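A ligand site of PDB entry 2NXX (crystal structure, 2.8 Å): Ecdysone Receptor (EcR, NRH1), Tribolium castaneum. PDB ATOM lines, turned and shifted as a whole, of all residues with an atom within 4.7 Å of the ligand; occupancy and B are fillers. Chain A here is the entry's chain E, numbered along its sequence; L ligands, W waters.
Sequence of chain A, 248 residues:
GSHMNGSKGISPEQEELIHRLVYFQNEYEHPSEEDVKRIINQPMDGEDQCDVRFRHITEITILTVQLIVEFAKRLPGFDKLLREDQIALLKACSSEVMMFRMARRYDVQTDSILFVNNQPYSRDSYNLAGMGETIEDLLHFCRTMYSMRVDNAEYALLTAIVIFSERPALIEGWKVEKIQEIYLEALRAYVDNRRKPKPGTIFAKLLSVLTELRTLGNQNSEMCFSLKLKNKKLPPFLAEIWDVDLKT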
ATOM      1  N   GLU A  29      31.363   4.232  24.383  1.00  0.00           N
ATOM      2  CA  GLU A  29      30.140   3.447  24.321  1.00  0.00           C
ATOM      3  C   GLU A  29      29.606   3.321  22.887  1.00  0.00           C
ATOM      4  O   GLU A  29      29.505   2.216  22.366  1.00  0.00           O
ATOM      5  CB  GLU A  29      29.067   4.056  25.236  1.00  0.00           C
ATOM      6  CG  GLU A  29      27.874   3.138  25.504  1.00  0.00           C
ATOM      7  CD  GLU A  29      26.969   2.977  24.278  1.00  0.00           C
ATOM      8  OE1 GLU A  29      26.288   1.936  24.179  1.00  0.00           O
ATOM      9  OE2 GLU A  29      26.929   3.899  23.430  1.00  0.00           O
ATOM     10  N   HIS A  30      29.287   4.452  22.247  1.00  0.00           N
ATOM     11  CA  HIS A  30      28.765   4.423  20.884  1.00  0.00           C
ATOM     12  C   HIS A  30      29.664   5.123  19.874  1.00  0.00           C
ATOM     13  O   HIS A  30      30.496   5.942  20.244  1.00  0.00           O
ATOM     14  CB  HIS A  30      27.362   5.032  20.849  1.00  0.00           C
ATOM     15  CG  HIS A  30      27.302   6.457  21.322  1.00  0.00           C
ATOM     16  ND1 HIS A  30      28.150   6.969  22.266  1.00  0.00           N
ATOM     17  CD2 HIS A  30      26.454   7.468  20.994  1.00  0.00           C
ATOM     18  CE1 HIS A  30      27.843   8.233  22.514  1.00  0.00           C
ATOM     19  NE2 HIS A  30      26.805   8.557  21.750  1.00  0.00           N
ATOM     20  N   PRO A  31      29.524   4.797  18.584  1.00  0.00           N
ATOM     21  CA  PRO A  31      30.331   5.382  17.500  1.00  0.00           C
ATOM     22  C   PRO A  31      29.904   6.785  17.077  1.00  0.00           C
ATOM     23  O   PRO A  31      28.872   7.303  17.508  1.00  0.00           O
ATOM     24  CB  PRO A  31      30.174   4.360  16.384  1.00  0.00           C
ATOM     25  CG  PRO A  31      28.784   3.930  16.564  1.00  0.00           C
ATOM     26  CD  PRO A  31      28.671   3.716  18.043  1.00  0.00           C
ATOM     27  N   ILE A  57      24.304  -4.698  10.279  1.00  0.00           N
ATOM     28  CA  ILE A  57      24.816  -5.427  11.405  1.00  0.00           C
ATOM     29  C   ILE A  57      26.329  -5.595  11.303  1.00  0.00           C
ATOM     30  O   ILE A  57      27.052  -5.270  12.233  1.00  0.00           O
ATOM     31  CB  ILE A  57      24.127  -6.806  11.523  1.00  0.00           C
ATOM     32  CG1 ILE A  57      22.687  -6.604  11.989  1.00  0.00           C
ATOM     33  CG2 ILE A  57      24.862  -7.686  12.533  1.00  0.00           C
ATOM     34  CD1 ILE A  57      21.931  -7.898  12.272  1.00  0.00           C
ATOM     35  N   THR A  58      26.830  -6.069  10.173  1.00  0.00           N
ATOM     36  CA  THR A  58      28.262  -6.268  10.048  1.00  0.00           C
ATOM     37  C   THR A  58      29.070  -4.974  10.072  1.00  0.00           C
ATOM     38  O   THR A  58      30.112  -4.904  10.711  1.00  0.00           O
ATOM     39  CB  THR A  58      28.632  -7.056   8.781  1.00  0.00           C
ATOM     40  OG1 THR A  58      28.060  -6.430   7.625  1.00  0.00           O
ATOM     41  CG2 THR A  58      28.121  -8.486   8.876  1.00  0.00           C
ATOM     42  N   ILE A  60      28.214  -1.923  11.351  1.00  0.00           N
ATOM     43  CA  ILE A  60      28.184  -1.297  12.663  1.00  0.00           C
ATOM     44  C   ILE A  60      29.090  -2.066  13.619  1.00  0.00           C
ATOM     45  O   ILE A  60      29.751  -1.470  14.442  1.00  0.00           O
ATOM     46  CB  ILE A  60      26.774  -1.269  13.259  1.00  0.00           C
ATOM     47  CG1 ILE A  60      25.797  -0.563  12.321  1.00  0.00           C
ATOM     48  CG2 ILE A  60      26.781  -0.508  14.574  1.00  0.00           C
ATOM     49  CD1 ILE A  60      24.339  -0.611  12.786  1.00  0.00           C
ATOM     50  N   THR A  61      29.133  -3.382  13.492  1.00  0.00           N
ATOM     51  CA  THR A  61      29.975  -4.198  14.359  1.00  0.00           C
ATOM     52  C   THR A  61      31.449  -3.820  14.198  1.00  0.00           C
ATOM     53  O   THR A  61      32.233  -3.902  15.155  1.00  0.00           O
ATOM     54  CB  THR A  61      29.786  -5.711  14.079  1.00  0.00           C
ATOM     55  OG1 THR A  61      28.476  -6.121  14.509  1.00  0.00           O
ATOM     56  CG2 THR A  61      30.816  -6.537  14.819  1.00  0.00           C
ATOM     57  N   THR A  64      32.041  -1.100  16.361  1.00  0.00           N
ATOM     58  CA  THR A  64      31.984  -1.650  17.698  1.00  0.00           C
ATOM     59  C   THR A  64      33.339  -2.226  18.125  1.00  0.00           C
ATOM     60  O   THR A  64      33.810  -1.976  19.244  1.00  0.00           O
ATOM     61  CB  THR A  64      30.943  -2.763  17.796  1.00  0.00           C
ATOM     62  OG1 THR A  64      29.664  -2.249  17.441  1.00  0.00           O
ATOM     63  CG2 THR A  64      30.887  -3.298  19.213  1.00  0.00           C
ATOM     64  N   MET A  98      32.293  -7.656  23.074  1.00  0.00           N
ATOM     65  CA  MET A  98      31.120  -7.129  22.392  1.00  0.00           C
ATOM     66  C   MET A  98      29.822  -7.649  22.954  1.00  0.00           C
ATOM     67  O   MET A  98      28.776  -7.035  22.775  1.00  0.00           O
ATOM     68  CB  MET A  98      31.172  -7.381  20.897  1.00  0.00           C
ATOM     69  CG  MET A  98      31.052  -8.812  20.482  1.00  0.00           C
ATOM     70  SD  MET A  98      30.915  -8.908  18.676  1.00  0.00           S
ATOM     71  CE  MET A  98      30.943 -10.686  18.409  1.00  0.00           C
ATOM     72  N   MET A  99      29.862  -8.763  23.650  1.00  0.00           N
ATOM     73  CA  MET A  99      28.621  -9.268  24.225  1.00  0.00           C
ATOM     74  C   MET A  99      28.209  -8.311  25.322  1.00  0.00           C
ATOM     75  O   MET A  99      27.011  -8.113  25.540  1.00  0.00           O
ATOM     76  CB  MET A  99      28.808 -10.685  24.803  1.00  0.00           C
ATOM     77  CG  MET A  99      29.258 -11.718  23.778  1.00  0.00           C
ATOM     78  SD  MET A  99      28.177 -11.789  22.365  1.00  0.00           S
ATOM     79  CE  MET A  99      29.146 -12.787  21.186  1.00  0.00           C
ATOM     80  N   ARG A 101      28.867  -5.022  25.411  1.00  0.00           N
ATOM     81  CA  ARG A 101      28.347  -3.856  24.724  1.00  0.00           C
ATOM     82  C   ARG A 101      26.922  -4.112  24.294  1.00  0.00           C
ATOM     83  O   ARG A 101      26.058  -3.240  24.420  1.00  0.00           O
ATOM     84  CB  ARG A 101      29.243  -3.488  23.549  1.00  0.00           C
ATOM     85  CG  ARG A 101      30.450  -2.655  23.978  1.00  0.00           C
ATOM     86  CD  ARG A 101      31.246  -2.227  22.800  1.00  0.00           C
ATOM     87  NE  ARG A 101      31.722  -0.844  22.886  1.00  0.00           N
ATOM     88  CZ  ARG A 101      32.789  -0.471  23.569  1.00  0.00           C
ATOM     89  NH1 ARG A 101      33.488  -1.382  24.231  1.00  0.00           N
ATOM     90  NH2 ARG A 101      33.173   0.793  23.590  1.00  0.00           N
ATOM     91  N   MET A 102      26.663  -5.323  23.807  1.00  0.00           N
ATOM     92  CA  MET A 102      25.320  -5.702  23.389  1.00  0.00           C
ATOM     93  C   MET A 102      24.353  -5.736  24.575  1.00  0.00           C
ATOM     94  O   MET A 102      23.289  -5.153  24.518  1.00  0.00           O
ATOM     95  CB  MET A 102      25.311  -7.076  22.722  1.00  0.00           C
ATOM     96  CG  MET A 102      23.919  -7.674  22.624  1.00  0.00           C
ATOM     97  SD  MET A 102      23.875  -9.314  21.865  1.00  0.00           S
ATOM     98  CE  MET A 102      24.651 -10.348  23.228  1.00  0.00           C
ATOM     99  N   ARG A 105      22.817  -2.595  25.808  1.00  0.00           N
ATOM    100  CA  ARG A 105      21.819  -1.931  24.971  1.00  0.00           C
ATOM    101  C   ARG A 105      20.575  -2.816  24.836  1.00  0.00           C
ATOM    102  O   ARG A 105      19.779  -2.664  23.898  1.00  0.00           O
ATOM    103  CB  ARG A 105      22.399  -1.638  23.585  1.00  0.00           C
ATOM    104  CG  ARG A 105      23.519  -0.632  23.600  1.00  0.00           C
ATOM    105  CD  ARG A 105      23.078   0.668  24.238  1.00  0.00           C
ATOM    106  NE  ARG A 105      22.188   1.434  23.362  1.00  0.00           N
ATOM    107  CZ  ARG A 105      22.573   2.073  22.258  1.00  0.00           C
ATOM    108  NH1 ARG A 105      23.858   2.033  21.871  1.00  0.00           N
ATOM    109  NH2 ARG A 105      21.692   2.737  21.520  1.00  0.00           N
ATOM    110  N   ILE A 113      17.564  -5.374  21.095  1.00  0.00           N
ATOM    111  CA  ILE A 113      18.770  -4.613  21.271  1.00  0.00           C
ATOM    112  C   ILE A 113      18.621  -3.272  20.554  1.00  0.00           C
ATOM    113  O   ILE A 113      18.253  -3.225  19.373  1.00  0.00           O
ATOM    114  CB  ILE A 113      19.977  -5.402  20.708  1.00  0.00           C
ATOM    115  CG1 ILE A 113      20.090  -6.744  21.445  1.00  0.00           C
ATOM    116  CG2 ILE A 113      21.250  -4.602  20.863  1.00  0.00           C
ATOM    117  CD1 ILE A 113      20.984  -7.725  20.753  1.00  0.00           C
ATOM    118  N   LEU A 114      18.877  -2.185  21.270  1.00  0.00           N
ATOM    119  CA  LEU A 114      18.768  -0.853  20.679  1.00  0.00           C
ATOM    120  C   LEU A 114      20.031  -0.469  19.951  1.00  0.00           C
ATOM    121  O   LEU A 114      20.999  -0.048  20.588  1.00  0.00           O
ATOM    122  CB  LEU A 114      18.512   0.200  21.760  1.00  0.00           C
ATOM    123  CG  LEU A 114      17.214   0.156  22.574  1.00  0.00           C
ATOM    124  CD1 LEU A 114      16.024   0.018  21.618  1.00  0.00           C
ATOM    125  CD2 LEU A 114      17.273  -0.996  23.576  1.00  0.00           C
ATOM    126  N   PHE A 115      20.044  -0.597  18.634  1.00  0.00           N
ATOM    127  CA  PHE A 115      21.220  -0.213  17.867  1.00  0.00           C
ATOM    128  C   PHE A 115      21.463   1.297  17.938  1.00  0.00           C
ATOM    129  O   PHE A 115      20.661   2.031  18.509  1.00  0.00           O
ATOM    130  CB  PHE A 115      21.067  -0.683  16.418  1.00  0.00           C
ATOM    131  CG  PHE A 115      21.367  -2.142  16.205  1.00  0.00           C
ATOM    132  CD1 PHE A 115      21.073  -3.071  17.197  1.00  0.00           C
ATOM    133  CD2 PHE A 115      21.915  -2.587  15.014  1.00  0.00           C
ATOM    134  CE1 PHE A 115      21.320  -4.424  16.998  1.00  0.00           C
ATOM    135  CE2 PHE A 115      22.165  -3.948  14.811  1.00  0.00           C
ATOM    136  CZ  PHE A 115      21.868  -4.864  15.799  1.00  0.00           C
ATOM    137  N   VAL A 116      22.573   1.737  17.365  1.00  0.00           N
ATOM    138  CA  VAL A 116      22.941   3.146  17.380  1.00  0.00           C
ATOM    139  C   VAL A 116      21.844   4.050  16.859  1.00  0.00           C
ATOM    140  O   VAL A 116      21.545   5.080  17.469  1.00  0.00           O
ATOM    141  CB  VAL A 116      24.194   3.398  16.514  1.00  0.00           C
ATOM    142  CG1 VAL A 116      24.595   4.864  16.599  1.00  0.00           C
ATOM    143  CG2 VAL A 116      25.331   2.536  16.991  1.00  0.00           C
ATOM    144  N   TYR A 126      17.463 -10.212  13.336  1.00  0.00           N
ATOM    145  CA  TYR A 126      18.667 -11.007  13.097  1.00  0.00           C
ATOM    146  C   TYR A 126      18.359 -12.144  12.139  1.00  0.00           C
ATOM    147  O   TYR A 126      19.169 -12.485  11.280  1.00  0.00           O
ATOM    148  CB  TYR A 126      19.225 -11.584  14.411  1.00  0.00           C
ATOM    149  CG  TYR A 126      20.038 -10.600  15.218  1.00  0.00           C
ATOM    150  CD1 TYR A 126      19.415  -9.651  16.021  1.00  0.00           C
ATOM    151  CD2 TYR A 126      21.429 -10.623  15.162  1.00  0.00           C
ATOM    152  CE1 TYR A 126      20.172  -8.732  16.774  1.00  0.00           C
ATOM    153  CE2 TYR A 126      22.190  -9.712  15.911  1.00  0.00           C
ATOM    154  CZ  TYR A 126      21.547  -8.773  16.719  1.00  0.00           C
ATOM    155  OH  TYR A 126      22.281  -7.888  17.474  1.00  0.00           O
ATOM    156  N   MET A 131      21.117 -14.441  10.595  1.00  0.00           N
ATOM    157  CA  MET A 131      21.818 -14.746  11.834  1.00  0.00           C
ATOM    158  C   MET A 131      20.852 -15.144  12.929  1.00  0.00           C
ATOM    159  O   MET A 131      21.011 -14.741  14.080  1.00  0.00           O
ATOM    160  CB  MET A 131      22.635 -13.545  12.293  1.00  0.00           C
ATOM    161  CG  MET A 131      23.561 -13.021  11.225  1.00  0.00           C
ATOM    162  SD  MET A 131      24.598 -11.716  11.862  1.00  0.00           S
ATOM    163  CE  MET A 131      26.136 -12.175  11.105  1.00  0.00           C
ATOM    164  N   LEU A 138      22.139 -15.247  22.351  1.00  0.00           N
ATOM    165  CA  LEU A 138      22.576 -13.879  22.542  1.00  0.00           C
ATOM    166  C   LEU A 138      21.595 -13.123  23.435  1.00  0.00           C
ATOM    167  O   LEU A 138      21.984 -12.519  24.437  1.00  0.00           O
ATOM    168  CB  LEU A 138      22.708 -13.200  21.181  1.00  0.00           C
ATOM    169  CG  LEU A 138      24.126 -12.933  20.671  1.00  0.00           C
ATOM    170  CD1 LEU A 138      25.124 -13.914  21.257  1.00  0.00           C
ATOM    171  CD2 LEU A 138      24.122 -13.006  19.165  1.00  0.00           C
ATOM    172  N   ASN A 220      30.145 -17.361  18.197  1.00  0.00           N
ATOM    173  CA  ASN A 220      30.342 -16.319  17.222  1.00  0.00           C
ATOM    174  C   ASN A 220      31.212 -16.862  16.079  1.00  0.00           C
ATOM    175  O   ASN A 220      30.939 -16.617  14.894  1.00  0.00           O
ATOM    176  CB  ASN A 220      31.026 -15.113  17.854  1.00  0.00           C
ATOM    177  CG  ASN A 220      31.149 -13.958  16.885  1.00  0.00           C
ATOM    178  OD1 ASN A 220      30.136 -13.393  16.456  1.00  0.00           O
ATOM    179  ND2 ASN A 220      32.392 -13.593  16.531  1.00  0.00           N
ATOM    180  N   MET A 223      29.275 -19.284  13.908  1.00  0.00           N
ATOM    181  CA  MET A 223      28.385 -18.600  12.983  1.00  0.00           C
ATOM    182  C   MET A 223      29.127 -17.974  11.805  1.00  0.00           C
ATOM    183  O   MET A 223      28.619 -17.968  10.686  1.00  0.00           O
ATOM    184  CB  MET A 223      27.603 -17.501  13.694  1.00  0.00           C
ATOM    185  CG  MET A 223      26.935 -16.592  12.681  1.00  0.00           C
ATOM    186  SD  MET A 223      25.862 -15.412  13.415  1.00  0.00           S
ATOM    187  CE  MET A 223      27.078 -14.403  14.385  1.00  0.00           C
ATOM    188  N   CYS A 224      30.301 -17.430  12.058  1.00  0.00           N
ATOM    189  CA  CYS A 224      31.077 -16.823  10.999  1.00  0.00           C
ATOM    190  C   CYS A 224      31.407 -17.860   9.942  1.00  0.00           C
ATOM    191  O   CYS A 224      31.273 -17.617   8.750  1.00  0.00           O
ATOM    192  CB  CYS A 224      32.343 -16.189  11.556  1.00  0.00           C
ATOM    193  SG  CYS A 224      32.063 -14.630  12.404  1.00  0.00           S
ATOM    194  N   LEU A 234      31.847 -12.080   5.224  1.00  0.00           N
ATOM    195  CA  LEU A 234      32.079 -11.330   6.436  1.00  0.00           C
ATOM    196  C   LEU A 234      33.044 -10.201   6.075  1.00  0.00           C
ATOM    197  O   LEU A 234      34.028 -10.431   5.349  1.00  0.00           O
ATOM    198  CB  LEU A 234      32.713 -12.253   7.474  1.00  0.00           C
ATOM    199  CG  LEU A 234      32.422 -12.133   8.972  1.00  0.00           C
ATOM    200  CD1 LEU A 234      33.710 -11.796   9.655  1.00  0.00           C
ATOM    201  CD2 LEU A 234      31.333 -11.113   9.281  1.00  0.00           C
ATOM    202  N   LEU A 238      36.557  -7.843  10.198  1.00  0.00           N
ATOM    203  CA  LEU A 238      36.051  -8.815  11.142  1.00  0.00           C
ATOM    204  C   LEU A 238      36.639 -10.204  10.878  1.00  0.00           C
ATOM    205  O   LEU A 238      37.124 -10.871  11.796  1.00  0.00           O
ATOM    206  CB  LEU A 238      34.523  -8.860  11.034  1.00  0.00           C
ATOM    207  CG  LEU A 238      33.677  -8.067  12.036  1.00  0.00           C
ATOM    208  CD1 LEU A 238      34.420  -6.856  12.533  1.00  0.00           C
ATOM    209  CD2 LEU A 238      32.355  -7.680  11.392  1.00  0.00           C
ATOM    210  N   TRP A 242      39.167 -11.761  13.841  1.00  0.00           N
ATOM    211  CA  TRP A 242      38.691 -12.988  14.469  1.00  0.00           C
ATOM    212  C   TRP A 242      39.282 -14.242  13.808  1.00  0.00           C
ATOM    213  O   TRP A 242      38.925 -15.359  14.181  1.00  0.00           O
ATOM    214  CB  TRP A 242      37.154 -13.049  14.421  1.00  0.00           C
ATOM    215  CG  TRP A 242      36.471 -12.010  15.240  1.00  0.00           C
ATOM    216  CD1 TRP A 242      36.968 -11.371  16.339  1.00  0.00           C
ATOM    217  CD2 TRP A 242      35.144 -11.488  15.051  1.00  0.00           C
ATOM    218  NE1 TRP A 242      36.043 -10.487  16.844  1.00  0.00           N
ATOM    219  CE2 TRP A 242      34.918 -10.541  16.081  1.00  0.00           C
ATOM    220  CE3 TRP A 242      34.135 -11.730  14.122  1.00  0.00           C
ATOM    221  CZ2 TRP A 242      33.713  -9.842  16.192  1.00  0.00           C
ATOM    222  CZ3 TRP A 242      32.940 -11.034  14.244  1.00  0.00           C
ATOM    223  CH2 TRP A 242      32.738 -10.103  15.276  1.00  0.00           C
HETATM  224  C1  LIG L   1      25.607  -0.654  18.981  1.00  0.00           C
HETATM  225  C2  LIG L   1      25.781  -1.890  19.996  1.00  0.00           C
HETATM  226  C3  LIG L   1      26.529  -1.407  21.257  1.00  0.00           C
HETATM  227  C4  LIG L   1      27.909  -0.837  20.893  1.00  0.00           C
HETATM  228  C5  LIG L   1      27.820   0.396  19.880  1.00  0.00           C
HETATM  229  C6  LIG L   1      27.046  -0.064  18.561  1.00  0.00           C
HETATM  230  C7  LIG L   1      26.611  -3.079  19.175  1.00  0.00           C
HETATM  231  C8  LIG L   1      24.383  -2.424  20.452  1.00  0.00           C
HETATM  232  C9  LIG L   1      26.796  -4.324  20.149  1.00  0.00           C
HETATM  233  C10 LIG L   1      25.794  -3.447  17.839  1.00  0.00           C
HETATM  234  C11 LIG L   1      26.842  -5.746  19.537  1.00  0.00           C
HETATM  235  C12 LIG L   1      25.944  -4.868  17.337  1.00  0.00           C
HETATM  236  C13 LIG L   1      25.769  -6.071  18.415  1.00  0.00           C
HETATM  237  C14 LIG L   1      24.300  -6.106  19.017  1.00  0.00           C
HETATM  238  C15 LIG L   1      26.053  -7.220  17.371  1.00  0.00           C
HETATM  239  O1  LIG L   1      27.317  -4.887  16.804  1.00  0.00           O
HETATM  240  C16 LIG L   1      25.164  -5.319  16.083  1.00  0.00           C
HETATM  241  C17 LIG L   1      25.975  -8.772  17.774  1.00  0.00           C
HETATM  242  C18 LIG L   1      25.167  -6.839  16.111  1.00  0.00           C
HETATM  243  C19 LIG L   1      26.308  -9.674  16.531  1.00  0.00           C
HETATM  244  O2  LIG L   1      24.617  -9.123  18.155  1.00  0.00           O
HETATM  245  C20 LIG L   1      26.891  -9.118  18.998  1.00  0.00           C
HETATM  246  C21 LIG L   1      24.870  -1.113  17.688  1.00  0.00           C
HETATM  247  C22 LIG L   1      24.997  -2.500  17.194  1.00  0.00           C
HETATM  248  O3  LIG L   1      27.093   1.508  20.461  1.00  0.00           O
HETATM  249  O4  LIG L   1      28.583  -0.413  22.080  1.00  0.00           O
HETATM  250  O5  LIG L   1      26.210 -11.019  16.964  1.00  0.00           O
HETATM  251  C23 LIG L   1      27.739  -9.503  15.880  1.00  0.00           C
HETATM  252  C24 LIG L   1      27.854 -10.459  14.688  1.00  0.00           C
HETATM  253  C25 LIG L   1      28.950 -10.307  13.742  1.00  0.00           C
HETATM  254  C26 LIG L   1      28.668  -9.053  12.815  1.00  0.00           C
HETATM  255  C27 LIG L   1      29.098 -11.550  12.915  1.00  0.00           C
HETATM  256  O6  LIG L   1      24.179  -0.347  17.067  1.00  0.00           O
HETATM  257  O   HOH W   1      27.815 -12.788  17.839  1.00  0.00           O
HETATM  258  O   HOH W   2      24.720 -12.344  15.183  1.00  0.00           O
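The guanidinium group of Arg 101 sits at hydrogen-bond distance from an oxygen (O4) of the ligand (3.3 Å). The side-chain sulfur of Met 102 lies within hydrogen-bond range of an oxygen (O2) of the ligand. The side-chain hydroxyl (OG1) of Thr 61 lies within hydrogen-bond range of an oxygen (O1) of the ligand (2.9 Å). An oxygen (O2) of the ligand sits at hydrogen-bond distance from the side-chain hydroxyl (OH) of Tyr 126 (2.7 Å). The backbone NH (N) of Val 116 lies within hydrogen-bond range of an oxygen (O6) of the ligand (2.6 Å). O4 of the ligand is in hydrogen-bond range of O of Glu 29, at 2.8 Å.
OE1 of Glu 29 is in salt-bridge range of NH1 of Arg 105. OG1 of Thr 61 sits at hydrogen-bond distance from O of Ile 57, at 2.8 Å. O of Arg 105 sits at hydrogen-bond distance from N of Leu 114 (2.8 Å). The backbone carbonyl oxygen (O) of Ile 60 is in hydrogen-bond range of the side-chain hydroxyl (OG1) of Thr 64. N of Met 131 sits at hydrogen-bond distance from O of Tyr 126 (2.8 Å). O of Phe 115 lies within hydrogen-bond range of NH2 of Arg 105 (3.3 Å).
Residues that only touch the ligand: Phe 115 (3.1 Å), His 30 (3.4 Å), Met 131 (3.5 Å), Arg 105 (3.6 Å), Thr 64 (3.6 Å), Ile 60 (3.6 Å), Leu 138 (3.6 Å), Pro 31 (3.6 Å), Ile 57 (3.7 Å), Met 223 (3.8 Å), Ile 113 (3.8 Å), Thr 58 (3.9 Å) and Met 98 (3.99 Å). The nearest printed residue that does not touch the ligand is Trp 242 (4.1 Å).
Water W1 lies within hydrogen-bond range of O5 of the ligand and OD1 of Asn 220. Water W2 lies within hydrogen-bond range of an oxygen (O5) of the ligand (2.7 Å), the side-chain sulfur (SD) of Met 131 (3.4 Å) and the side-chain sulfur (SD) of Met 223 (3.7 Å).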
